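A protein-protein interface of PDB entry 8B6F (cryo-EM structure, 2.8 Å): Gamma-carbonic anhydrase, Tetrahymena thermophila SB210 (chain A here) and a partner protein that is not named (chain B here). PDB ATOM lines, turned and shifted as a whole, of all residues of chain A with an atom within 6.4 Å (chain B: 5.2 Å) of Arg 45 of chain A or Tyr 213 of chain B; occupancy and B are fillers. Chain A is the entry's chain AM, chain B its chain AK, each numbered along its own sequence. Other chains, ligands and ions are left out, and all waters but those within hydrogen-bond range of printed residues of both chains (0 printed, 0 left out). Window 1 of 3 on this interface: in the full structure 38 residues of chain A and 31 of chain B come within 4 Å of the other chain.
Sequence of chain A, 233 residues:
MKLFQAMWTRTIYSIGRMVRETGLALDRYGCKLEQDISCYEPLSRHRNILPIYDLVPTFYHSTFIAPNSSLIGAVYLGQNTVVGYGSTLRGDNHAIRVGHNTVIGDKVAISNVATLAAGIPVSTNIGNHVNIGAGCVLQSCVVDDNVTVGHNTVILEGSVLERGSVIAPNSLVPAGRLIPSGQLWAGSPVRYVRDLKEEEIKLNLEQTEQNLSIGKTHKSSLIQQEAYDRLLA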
ATOM      1  N   ARG A  17      -8.301  -4.219 -33.372  1.00  0.00           N
ATOM      2  CA  ARG A  17      -8.992  -5.323 -32.718  1.00  0.00           C
ATOM      3  C   ARG A  17      -8.012  -6.416 -32.315  1.00  0.00           C
ATOM      4  O   ARG A  17      -8.109  -6.974 -31.216  1.00  0.00           O
ATOM      5  CB  ARG A  17     -10.075  -5.885 -33.636  1.00  0.00           C
ATOM      6  CG  ARG A  17     -11.107  -6.722 -32.903  1.00  0.00           C
ATOM      7  CD  ARG A  17     -12.215  -7.183 -33.831  1.00  0.00           C
ATOM      8  NE  ARG A  17     -13.301  -7.825 -33.100  1.00  0.00           N
ATOM      9  CZ  ARG A  17     -13.341  -9.112 -32.783  1.00  0.00           C
ATOM     10  NH1 ARG A  17     -12.363  -9.938 -33.114  1.00  0.00           N
ATOM     11  NH2 ARG A  17     -14.393  -9.584 -32.120  1.00  0.00           N
ATOM     12  N   GLU A  21      -7.199  -7.795 -28.593  1.00  0.00           N
ATOM     13  CA  GLU A  21      -7.273  -9.213 -28.261  1.00  0.00           C
ATOM     14  C   GLU A  21      -6.004  -9.677 -27.561  1.00  0.00           C
ATOM     15  O   GLU A  21      -6.062 -10.307 -26.500  1.00  0.00           O
ATOM     16  CB  GLU A  21      -7.510 -10.030 -29.531  1.00  0.00           C
ATOM     17  CG  GLU A  21      -8.892  -9.861 -30.142  1.00  0.00           C
ATOM     18  CD  GLU A  21      -9.947 -10.696 -29.443  1.00  0.00           C
ATOM     19  OE1 GLU A  21      -9.714 -11.106 -28.287  1.00  0.00           O
ATOM     20  OE2 GLU A  21     -11.006 -10.949 -30.055  1.00  0.00           O
ATOM     21  N   LEU A  43     -19.357  -9.337 -15.047  1.00  0.00           N
ATOM     22  CA  LEU A  43     -19.950  -8.023 -14.917  1.00  0.00           C
ATOM     23  C   LEU A  43     -20.743  -7.760 -16.183  1.00  0.00           C
ATOM     24  O   LEU A  43     -20.408  -8.280 -17.249  1.00  0.00           O
ATOM     25  CB  LEU A  43     -18.844  -6.980 -14.728  1.00  0.00           C
ATOM     26  CG  LEU A  43     -18.301  -6.859 -13.302  1.00  0.00           C
ATOM     27  CD1 LEU A  43     -16.846  -6.421 -13.334  1.00  0.00           C
ATOM     28  CD2 LEU A  43     -19.114  -5.885 -12.477  1.00  0.00           C
ATOM     29  N   SER A  44     -21.800  -6.961 -16.075  1.00  0.00           N
ATOM     30  CA  SER A  44     -22.663  -6.809 -17.233  1.00  0.00           C
ATOM     31  C   SER A  44     -21.849  -6.218 -18.368  1.00  0.00           C
ATOM     32  O   SER A  44     -21.068  -5.284 -18.176  1.00  0.00           O
ATOM     33  CB  SER A  44     -23.865  -5.910 -16.934  1.00  0.00           C
ATOM     34  OG  SER A  44     -23.667  -5.126 -15.774  1.00  0.00           O
ATOM     35  N   ARG A  45     -22.034  -6.771 -19.558  1.00  0.00           N
ATOM     36  CA  ARG A  45     -21.308  -6.311 -20.724  1.00  0.00           C
ATOM     37  C   ARG A  45     -22.140  -5.302 -21.488  1.00  0.00           C
ATOM     38  O   ARG A  45     -21.731  -4.850 -22.560  1.00  0.00           O
ATOM     39  CB  ARG A  45     -20.928  -7.500 -21.614  1.00  0.00           C
ATOM     40  CG  ARG A  45     -19.964  -8.456 -20.920  1.00  0.00           C
ATOM     41  CD  ARG A  45     -19.148  -9.292 -21.888  1.00  0.00           C
ATOM     42  NE  ARG A  45     -18.165  -8.492 -22.608  1.00  0.00           N
ATOM     43  CZ  ARG A  45     -17.436  -8.933 -23.623  1.00  0.00           C
ATOM     44  NH1 ARG A  45     -17.554 -10.172 -24.071  1.00  0.00           N
ATOM     45  NH2 ARG A  45     -16.562  -8.114 -24.197  1.00  0.00           N
ATOM     46  N   HIS A  46     -23.305  -4.953 -20.942  1.00  0.00           N
ATOM     47  CA  HIS A  46     -24.227  -4.061 -21.617  1.00  0.00           C
ATOM     48  C   HIS A  46     -23.580  -2.713 -21.866  1.00  0.00           C
ATOM     49  O   HIS A  46     -22.935  -2.144 -20.982  1.00  0.00           O
ATOM     50  CB  HIS A  46     -25.482  -3.862 -20.776  1.00  0.00           C
ATOM     51  CG  HIS A  46     -26.553  -3.096 -21.483  1.00  0.00           C
ATOM     52  ND1 HIS A  46     -27.144  -1.974 -20.941  1.00  0.00           N
ATOM     53  CD2 HIS A  46     -27.141  -3.285 -22.686  1.00  0.00           C
ATOM     54  CE1 HIS A  46     -28.049  -1.508 -21.780  1.00  0.00           C
ATOM     55  NE2 HIS A  46     -28.067  -2.284 -22.848  1.00  0.00           N
ATOM     56  N   ARG A  47     -23.758  -2.207 -23.074  1.00  0.00           N
ATOM     57  CA  ARG A  47     -23.215  -0.927 -23.482  1.00  0.00           C
ATOM     58  C   ARG A  47     -24.391  -0.047 -23.866  1.00  0.00           C
ATOM     59  O   ARG A  47     -25.214  -0.450 -24.693  1.00  0.00           O
ATOM     60  CB  ARG A  47     -22.243  -1.116 -24.645  1.00  0.00           C
ATOM     61  CG  ARG A  47     -21.398  -2.375 -24.486  1.00  0.00           C
ATOM     62  CD  ARG A  47     -20.254  -2.449 -25.477  1.00  0.00           C
ATOM     63  NE  ARG A  47     -19.356  -3.557 -25.172  1.00  0.00           N
ATOM     64  CZ  ARG A  47     -18.451  -4.043 -26.010  1.00  0.00           C
ATOM     65  NH1 ARG A  47     -18.295  -3.542 -27.225  1.00  0.00           N
ATOM     66  NH2 ARG A  47     -17.681  -5.054 -25.620  1.00  0.00           N
ATOM     67  N   LEU A  50     -23.898   1.314 -28.464  1.00  0.00           N
ATOM     68  CA  LEU A  50     -23.129   0.274 -29.125  1.00  0.00           C
ATOM     69  C   LEU A  50     -22.995   0.678 -30.579  1.00  0.00           C
ATOM     70  O   LEU A  50     -24.022   0.899 -31.245  1.00  0.00           O
ATOM     71  CB  LEU A  50     -23.829  -1.082 -29.011  1.00  0.00           C
ATOM     72  CG  LEU A  50     -23.189  -2.253 -29.760  1.00  0.00           C
ATOM     73  CD1 LEU A  50     -21.858  -2.615 -29.144  1.00  0.00           C
ATOM     74  CD2 LEU A  50     -24.107  -3.460 -29.804  1.00  0.00           C
ATOM     75  N   TYR B  55     -27.357 -15.536 -29.739  1.00  0.00           N
ATOM     76  CA  TYR B  55     -26.985 -14.269 -29.124  1.00  0.00           C
ATOM     77  C   TYR B  55     -28.010 -13.907 -28.058  1.00  0.00           C
ATOM     78  O   TYR B  55     -29.197 -13.751 -28.362  1.00  0.00           O
ATOM     79  CB  TYR B  55     -26.891 -13.166 -30.179  1.00  0.00           C
ATOM     80  CG  TYR B  55     -26.612 -11.790 -29.620  1.00  0.00           C
ATOM     81  CD1 TYR B  55     -25.349 -11.445 -29.167  1.00  0.00           C
ATOM     82  CD2 TYR B  55     -27.612 -10.830 -29.565  1.00  0.00           C
ATOM     83  CE1 TYR B  55     -25.091 -10.188 -28.662  1.00  0.00           C
ATOM     84  CE2 TYR B  55     -27.364  -9.570 -29.063  1.00  0.00           C
ATOM     85  CZ  TYR B  55     -26.102  -9.256 -28.613  1.00  0.00           C
ATOM     86  OH  TYR B  55     -25.850  -8.001 -28.113  1.00  0.00           O
ATOM     87  N   PRO B  58     -26.919  -8.558 -23.396  1.00  0.00           N
ATOM     88  CA  PRO B  58     -26.529  -8.350 -21.991  1.00  0.00           C
ATOM     89  C   PRO B  58     -27.671  -7.853 -21.123  1.00  0.00           C
ATOM     90  O   PRO B  58     -27.755  -8.218 -19.945  1.00  0.00           O
ATOM     91  CB  PRO B  58     -25.396  -7.320 -22.093  1.00  0.00           C
ATOM     92  CG  PRO B  58     -24.867  -7.469 -23.469  1.00  0.00           C
ATOM     93  CD  PRO B  58     -26.043  -7.818 -24.321  1.00  0.00           C
ATOM     94  N   TYR B  76     -32.732  -7.242 -26.529  1.00  0.00           N
ATOM     95  CA  TYR B  76     -32.428  -6.555 -25.283  1.00  0.00           C
ATOM     96  C   TYR B  76     -33.667  -6.395 -24.412  1.00  0.00           C
ATOM     97  O   TYR B  76     -34.771  -6.153 -24.910  1.00  0.00           O
ATOM     98  CB  TYR B  76     -31.819  -5.183 -25.583  1.00  0.00           C
ATOM     99  CG  TYR B  76     -30.550  -5.256 -26.401  1.00  0.00           C
ATOM    100  CD1 TYR B  76     -30.597  -5.453 -27.775  1.00  0.00           C
ATOM    101  CD2 TYR B  76     -29.307  -5.120 -25.802  1.00  0.00           C
ATOM    102  CE1 TYR B  76     -29.443  -5.521 -28.526  1.00  0.00           C
ATOM    103  CE2 TYR B  76     -28.146  -5.188 -26.545  1.00  0.00           C
ATOM    104  CZ  TYR B  76     -28.222  -5.389 -27.906  1.00  0.00           C
ATOM    105  OH  TYR B  76     -27.067  -5.454 -28.649  1.00  0.00           O
ATOM    106  N   HIS B 209     -24.506  -7.813 -34.385  1.00  0.00           N
ATOM    107  CA  HIS B 209     -24.466  -7.391 -32.990  1.00  0.00           C
ATOM    108  C   HIS B 209     -23.410  -8.170 -32.220  1.00  0.00           C
ATOM    109  O   HIS B 209     -22.679  -7.605 -31.401  1.00  0.00           O
ATOM    110  CB  HIS B 209     -25.836  -7.604 -32.350  1.00  0.00           C
ATOM    111  CG  HIS B 209     -26.847  -6.562 -32.707  1.00  0.00           C
ATOM    112  ND1 HIS B 209     -27.194  -5.537 -31.855  1.00  0.00           N
ATOM    113  CD2 HIS B 209     -27.582  -6.382 -33.829  1.00  0.00           C
ATOM    114  CE1 HIS B 209     -28.111  -4.781 -32.432  1.00  0.00           C
ATOM    115  NE2 HIS B 209     -28.360  -5.269 -33.632  1.00  0.00           N
ATOM    116  N   ARG B 210     -23.318  -9.476 -32.480  1.00  0.00           N
ATOM    117  CA  ARG B 210     -22.375 -10.325 -31.762  1.00  0.00           C
ATOM    118  C   ARG B 210     -20.937  -9.872 -31.980  1.00  0.00           C
ATOM    119  O   ARG B 210     -20.129  -9.871 -31.045  1.00  0.00           O
ATOM    120  CB  ARG B 210     -22.558 -11.772 -32.220  1.00  0.00           C
ATOM    121  CG  ARG B 210     -21.706 -12.798 -31.499  1.00  0.00           C
ATOM    122  CD  ARG B 210     -21.574 -14.055 -32.346  1.00  0.00           C
ATOM    123  NE  ARG B 210     -21.443 -15.260 -31.537  1.00  0.00           N
ATOM    124  CZ  ARG B 210     -22.463 -15.956 -31.055  1.00  0.00           C
ATOM    125  NH1 ARG B 210     -23.715 -15.584 -31.265  1.00  0.00           N
ATOM    126  NH2 ARG B 210     -22.222 -17.051 -30.341  1.00  0.00           N
ATOM    127  N   TYR B 211     -20.600  -9.486 -33.212  1.00  0.00           N
ATOM    128  CA  TYR B 211     -19.215  -9.187 -33.552  1.00  0.00           C
ATOM    129  C   TYR B 211     -18.663  -8.000 -32.776  1.00  0.00           C
ATOM    130  O   TYR B 211     -17.442  -7.817 -32.732  1.00  0.00           O
ATOM    131  CB  TYR B 211     -19.104  -8.928 -35.055  1.00  0.00           C
ATOM    132  CG  TYR B 211     -17.707  -8.589 -35.519  1.00  0.00           C
ATOM    133  CD1 TYR B 211     -16.712  -9.557 -35.559  1.00  0.00           C
ATOM    134  CD2 TYR B 211     -17.387  -7.303 -35.924  1.00  0.00           C
ATOM    135  CE1 TYR B 211     -15.437  -9.249 -35.983  1.00  0.00           C
ATOM    136  CE2 TYR B 211     -16.115  -6.985 -36.350  1.00  0.00           C
ATOM    137  CZ  TYR B 211     -15.145  -7.961 -36.377  1.00  0.00           C
ATOM    138  OH  TYR B 211     -13.877  -7.648 -36.803  1.00  0.00           O
ATOM    139  N   GLU B 212     -19.525  -7.195 -32.160  1.00  0.00           N
ATOM    140  CA  GLU B 212     -19.074  -5.991 -31.476  1.00  0.00           C
ATOM    141  C   GLU B 212     -18.465  -6.259 -30.106  1.00  0.00           C
ATOM    142  O   GLU B 212     -17.874  -5.341 -29.526  1.00  0.00           O
ATOM    143  CB  GLU B 212     -20.241  -5.015 -31.325  1.00  0.00           C
ATOM    144  CG  GLU B 212     -20.609  -4.287 -32.608  1.00  0.00           C
ATOM    145  CD  GLU B 212     -19.537  -3.308 -33.051  1.00  0.00           C
ATOM    146  OE1 GLU B 212     -18.730  -2.881 -32.201  1.00  0.00           O
ATOM    147  OE2 GLU B 212     -19.498  -2.970 -34.252  1.00  0.00           O
ATOM    148  N   TYR B 213     -18.588  -7.471 -29.574  1.00  0.00           N
ATOM    149  CA  TYR B 213     -18.070  -7.810 -28.256  1.00  0.00           C
ATOM    150  C   TYR B 213     -16.840  -8.693 -28.399  1.00  0.00           C
ATOM    151  O   TYR B 213     -16.882  -9.715 -29.090  1.00  0.00           O
ATOM    152  CB  TYR B 213     -19.131  -8.524 -27.416  1.00  0.00           C
ATOM    153  CG  TYR B 213     -20.324  -7.662 -27.077  1.00  0.00           C
ATOM    154  CD1 TYR B 213     -21.420  -7.591 -27.925  1.00  0.00           C
ATOM    155  CD2 TYR B 213     -20.354  -6.922 -25.906  1.00  0.00           C
ATOM    156  CE1 TYR B 213     -22.510  -6.806 -27.615  1.00  0.00           C
ATOM    157  CE2 TYR B 213     -21.439  -6.134 -25.587  1.00  0.00           C
ATOM    158  CZ  TYR B 213     -22.513  -6.078 -26.446  1.00  0.00           C
ATOM    159  OH  TYR B 213     -23.598  -5.293 -26.130  1.00  0.00           O
ATOM    160  N   LEU B 214     -15.752  -8.296 -27.751  1.00  0.00           N
ATOM    161  CA  LEU B 214     -14.562  -9.128 -27.726  1.00  0.00           C
ATOM    162  C   LEU B 214     -14.744 -10.281 -26.742  1.00  0.00           C
ATOM    163  O   LEU B 214     -15.516 -10.175 -25.786  1.00  0.00           O
ATOM    164  CB  LEU B 214     -13.342  -8.302 -27.334  1.00  0.00           C
ATOM    165  CG  LEU B 214     -12.880  -7.241 -28.337  1.00  0.00           C
ATOM    166  CD1 LEU B 214     -11.659  -6.516 -27.805  1.00  0.00           C
ATOM    167  CD2 LEU B 214     -12.577  -7.847 -29.696  1.00  0.00           C
ATOM    168  N   PRO B 215     -14.040 -11.395 -26.951  1.00  0.00           N
ATOM    169  CA  PRO B 215     -14.217 -12.549 -26.052  1.00  0.00           C
ATOM    170  C   PRO B 215     -13.803 -12.280 -24.618  1.00  0.00           C
ATOM    171  O   PRO B 215     -14.233 -13.014 -23.721  1.00  0.00           O
ATOM    172  CB  PRO B 215     -13.341 -13.632 -26.697  1.00  0.00           C
ATOM    173  CG  PRO B 215     -12.331 -12.884 -27.481  1.00  0.00           C
ATOM    174  CD  PRO B 215     -13.028 -11.658 -27.987  1.00  0.00           C
ATOM    175  N   TYR B 216     -12.983 -11.263 -24.368  1.00  0.00           N
ATOM    176  CA  TYR B 216     -12.502 -10.941 -23.031  1.00  0.00           C
ATOM    177  C   TYR B 216     -13.207  -9.683 -22.544  1.00  0.00           C
ATOM    178  O   TYR B 216     -13.151  -8.641 -23.205  1.00  0.00           O
ATOM    179  CB  TYR B 216     -10.988 -10.738 -23.030  1.00  0.00           C
ATOM    180  CG  TYR B 216     -10.218 -11.878 -23.653  1.00  0.00           C
ATOM    181  CD1 TYR B 216     -10.001 -13.058 -22.957  1.00  0.00           C
ATOM    182  CD2 TYR B 216      -9.700 -11.766 -24.935  1.00  0.00           C
ATOM    183  CE1 TYR B 216      -9.293 -14.099 -23.523  1.00  0.00           C
ATOM    184  CE2 TYR B 216      -8.992 -12.800 -25.511  1.00  0.00           C
ATOM    185  CZ  TYR B 216      -8.792 -13.965 -24.801  1.00  0.00           C
ATOM    186  OH  TYR B 216      -8.086 -14.998 -25.372  1.00  0.00           O
ATOM    187  N   ASN B 217     -13.868  -9.782 -21.395  1.00  0.00           N
ATOM    188  CA  ASN B 217     -14.541  -8.636 -20.799  1.00  0.00           C
ATOM    189  C   ASN B 217     -13.513  -7.724 -20.139  1.00  0.00           C
ATOM    190  O   ASN B 217     -12.640  -8.191 -19.403  1.00  0.00           O
ATOM    191  CB  ASN B 217     -15.575  -9.106 -19.778  1.00  0.00           C
ATOM    192  CG  ASN B 217     -16.428  -7.975 -19.245  1.00  0.00           C
ATOM    193  OD1 ASN B 217     -16.111  -6.802 -19.429  1.00  0.00           O
ATOM    194  ND2 ASN B 217     -17.517  -8.326 -18.575  1.00  0.00           N
ATOM    195  N   SER B 218     -13.617  -6.423 -20.405  1.00  0.00           N
ATOM    196  CA  SER B 218     -12.692  -5.435 -19.865  1.00  0.00           C
ATOM    197  C   SER B 218     -13.312  -4.586 -18.763  1.00  0.00           C
ATOM    198  O   SER B 218     -12.700  -3.605 -18.333  1.00  0.00           O
ATOM    199  CB  SER B 218     -12.176  -4.532 -20.985  1.00  0.00           C
ATOM    200  OG  SER B 218     -13.240  -3.836 -21.608  1.00  0.00           O
ATOM    201  N   PRO B 254     -18.758 -14.462 -27.700  1.00  0.00           N
ATOM    202  CA  PRO B 254     -18.002 -13.496 -26.888  1.00  0.00           C
ATOM    203  C   PRO B 254     -18.600 -13.257 -25.513  1.00  0.00           C
ATOM    204  O   PRO B 254     -17.855 -12.977 -24.566  1.00  0.00           O
ATOM    205  CB  PRO B 254     -18.023 -12.225 -27.748  1.00  0.00           C
ATOM    206  CG  PRO B 254     -19.205 -12.372 -28.621  1.00  0.00           C
ATOM    207  CD  PRO B 254     -19.331 -13.835 -28.903  1.00  0.00           C
ATOM    208  N   LEU B 255     -19.919 -13.356 -25.371  1.00  0.00           N
ATOM    209  CA  LEU B 255     -20.587 -13.100 -24.095  1.00  0.00           C
ATOM    210  C   LEU B 255     -20.599 -14.341 -23.210  1.00  0.00           C
ATOM    211  O   LEU B 255     -21.641 -14.768 -22.717  1.00  0.00           O
ATOM    212  CB  LEU B 255     -22.005 -12.603 -24.348  1.00  0.00           C
ATOM    213  CG  LEU B 255     -22.143 -11.397 -25.277  1.00  0.00           C
ATOM    214  CD1 LEU B 255     -23.607 -11.071 -25.501  1.00  0.00           C
ATOM    215  CD2 LEU B 255     -21.409 -10.197 -24.715  1.00  0.00           C
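Arg 45 of chain A touches seven residues of chain B.
Tyr 213 of chain B touches three residues of chain A.
Of the printed residues of chain A, Tyr 211 of chain B touches Arg 17 (3.4 Å).
Printed residues of chain A within 4 Å of Asn 217 of chain B: Leu 43 and Arg 45.
Of the printed residues of chain A, Pro 215 of chain B touches Glu 21.
Arg 210 of chain B touches none of the printed residues of chain A.
Ser 44 of chain A touches none of the printed residues of chain B.
The nearest residue of chain A that does not touch Tyr 213 of chain B is Leu 50 of chain A (4.1 Å).
OH of Tyr 55 of chain B sits at hydrogen-bond distance from OH of Tyr 76 of chain B, at 2.9 Å.
NH1 of Arg 17 of chain A is in salt-bridge range of OE2 of Glu 21 of chain A (3.5 Å).
ND1 of His 209 of chain B lies within hydrogen-bond range of OH of Tyr 76 of chain B, at 3.2 Å.
Arg 17 of chain A touches Tyr 211 of chain B (CD to OH, 3.4 Å).
Arg 17 of chain A touches Leu 214 of chain B (CZ to CD2, 3.4 Å).
OE2 of Glu 21 of chain A touches CD2 of Leu 214 of chain B, 3.5 Å away.
Arg 45 of chain A touches Pro 58 of chain B.
O of Arg 45 of chain A touches CE2 of Tyr 213 of chain B (3.3 Å).
Tyr 216 of chain B touches Arg 45 of chain A.
CD of Arg 45 of chain A touches CD2 of Leu 255 of chain B (3.7 Å).
His 46 of chain A touches Pro 58 of chain B (N to CB, 3.4 Å).
Arg 47 of chain A touches Tyr 213 of chain B.
CD2 of Leu 50 of chain A touches OH of Tyr 76 of chain B, 3.8 Å away.
Hydrophobic or aromatic side chains of chain B that line the printed part of chain A: Pro 58, Tyr 76, Tyr 211, Tyr 213, Leu 214, Pro 215, Tyr 216 and Leu 255.
Of the 8 printed residues of chain A, 7 touch a printed residue of chain B.
Among the printed residues, 19 pairs touch across the chains.
O of Leu 214 of chain B lies within hydrogen-bond range of NH1 of Arg 45 of chain A (2.7 Å).
NH1 of Arg 45 of chain A is in hydrogen-bond range of O of Pro 254 of chain B, 2.9 Å away.
ND2 of Asn 217 of chain B lies within hydrogen-bond range of O of Leu 43 of chain A, 3.2 Å away.
O of Glu 212 of chain B sits at hydrogen-bond distance from NH1 of Arg 47 of chain A (3.0 Å).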
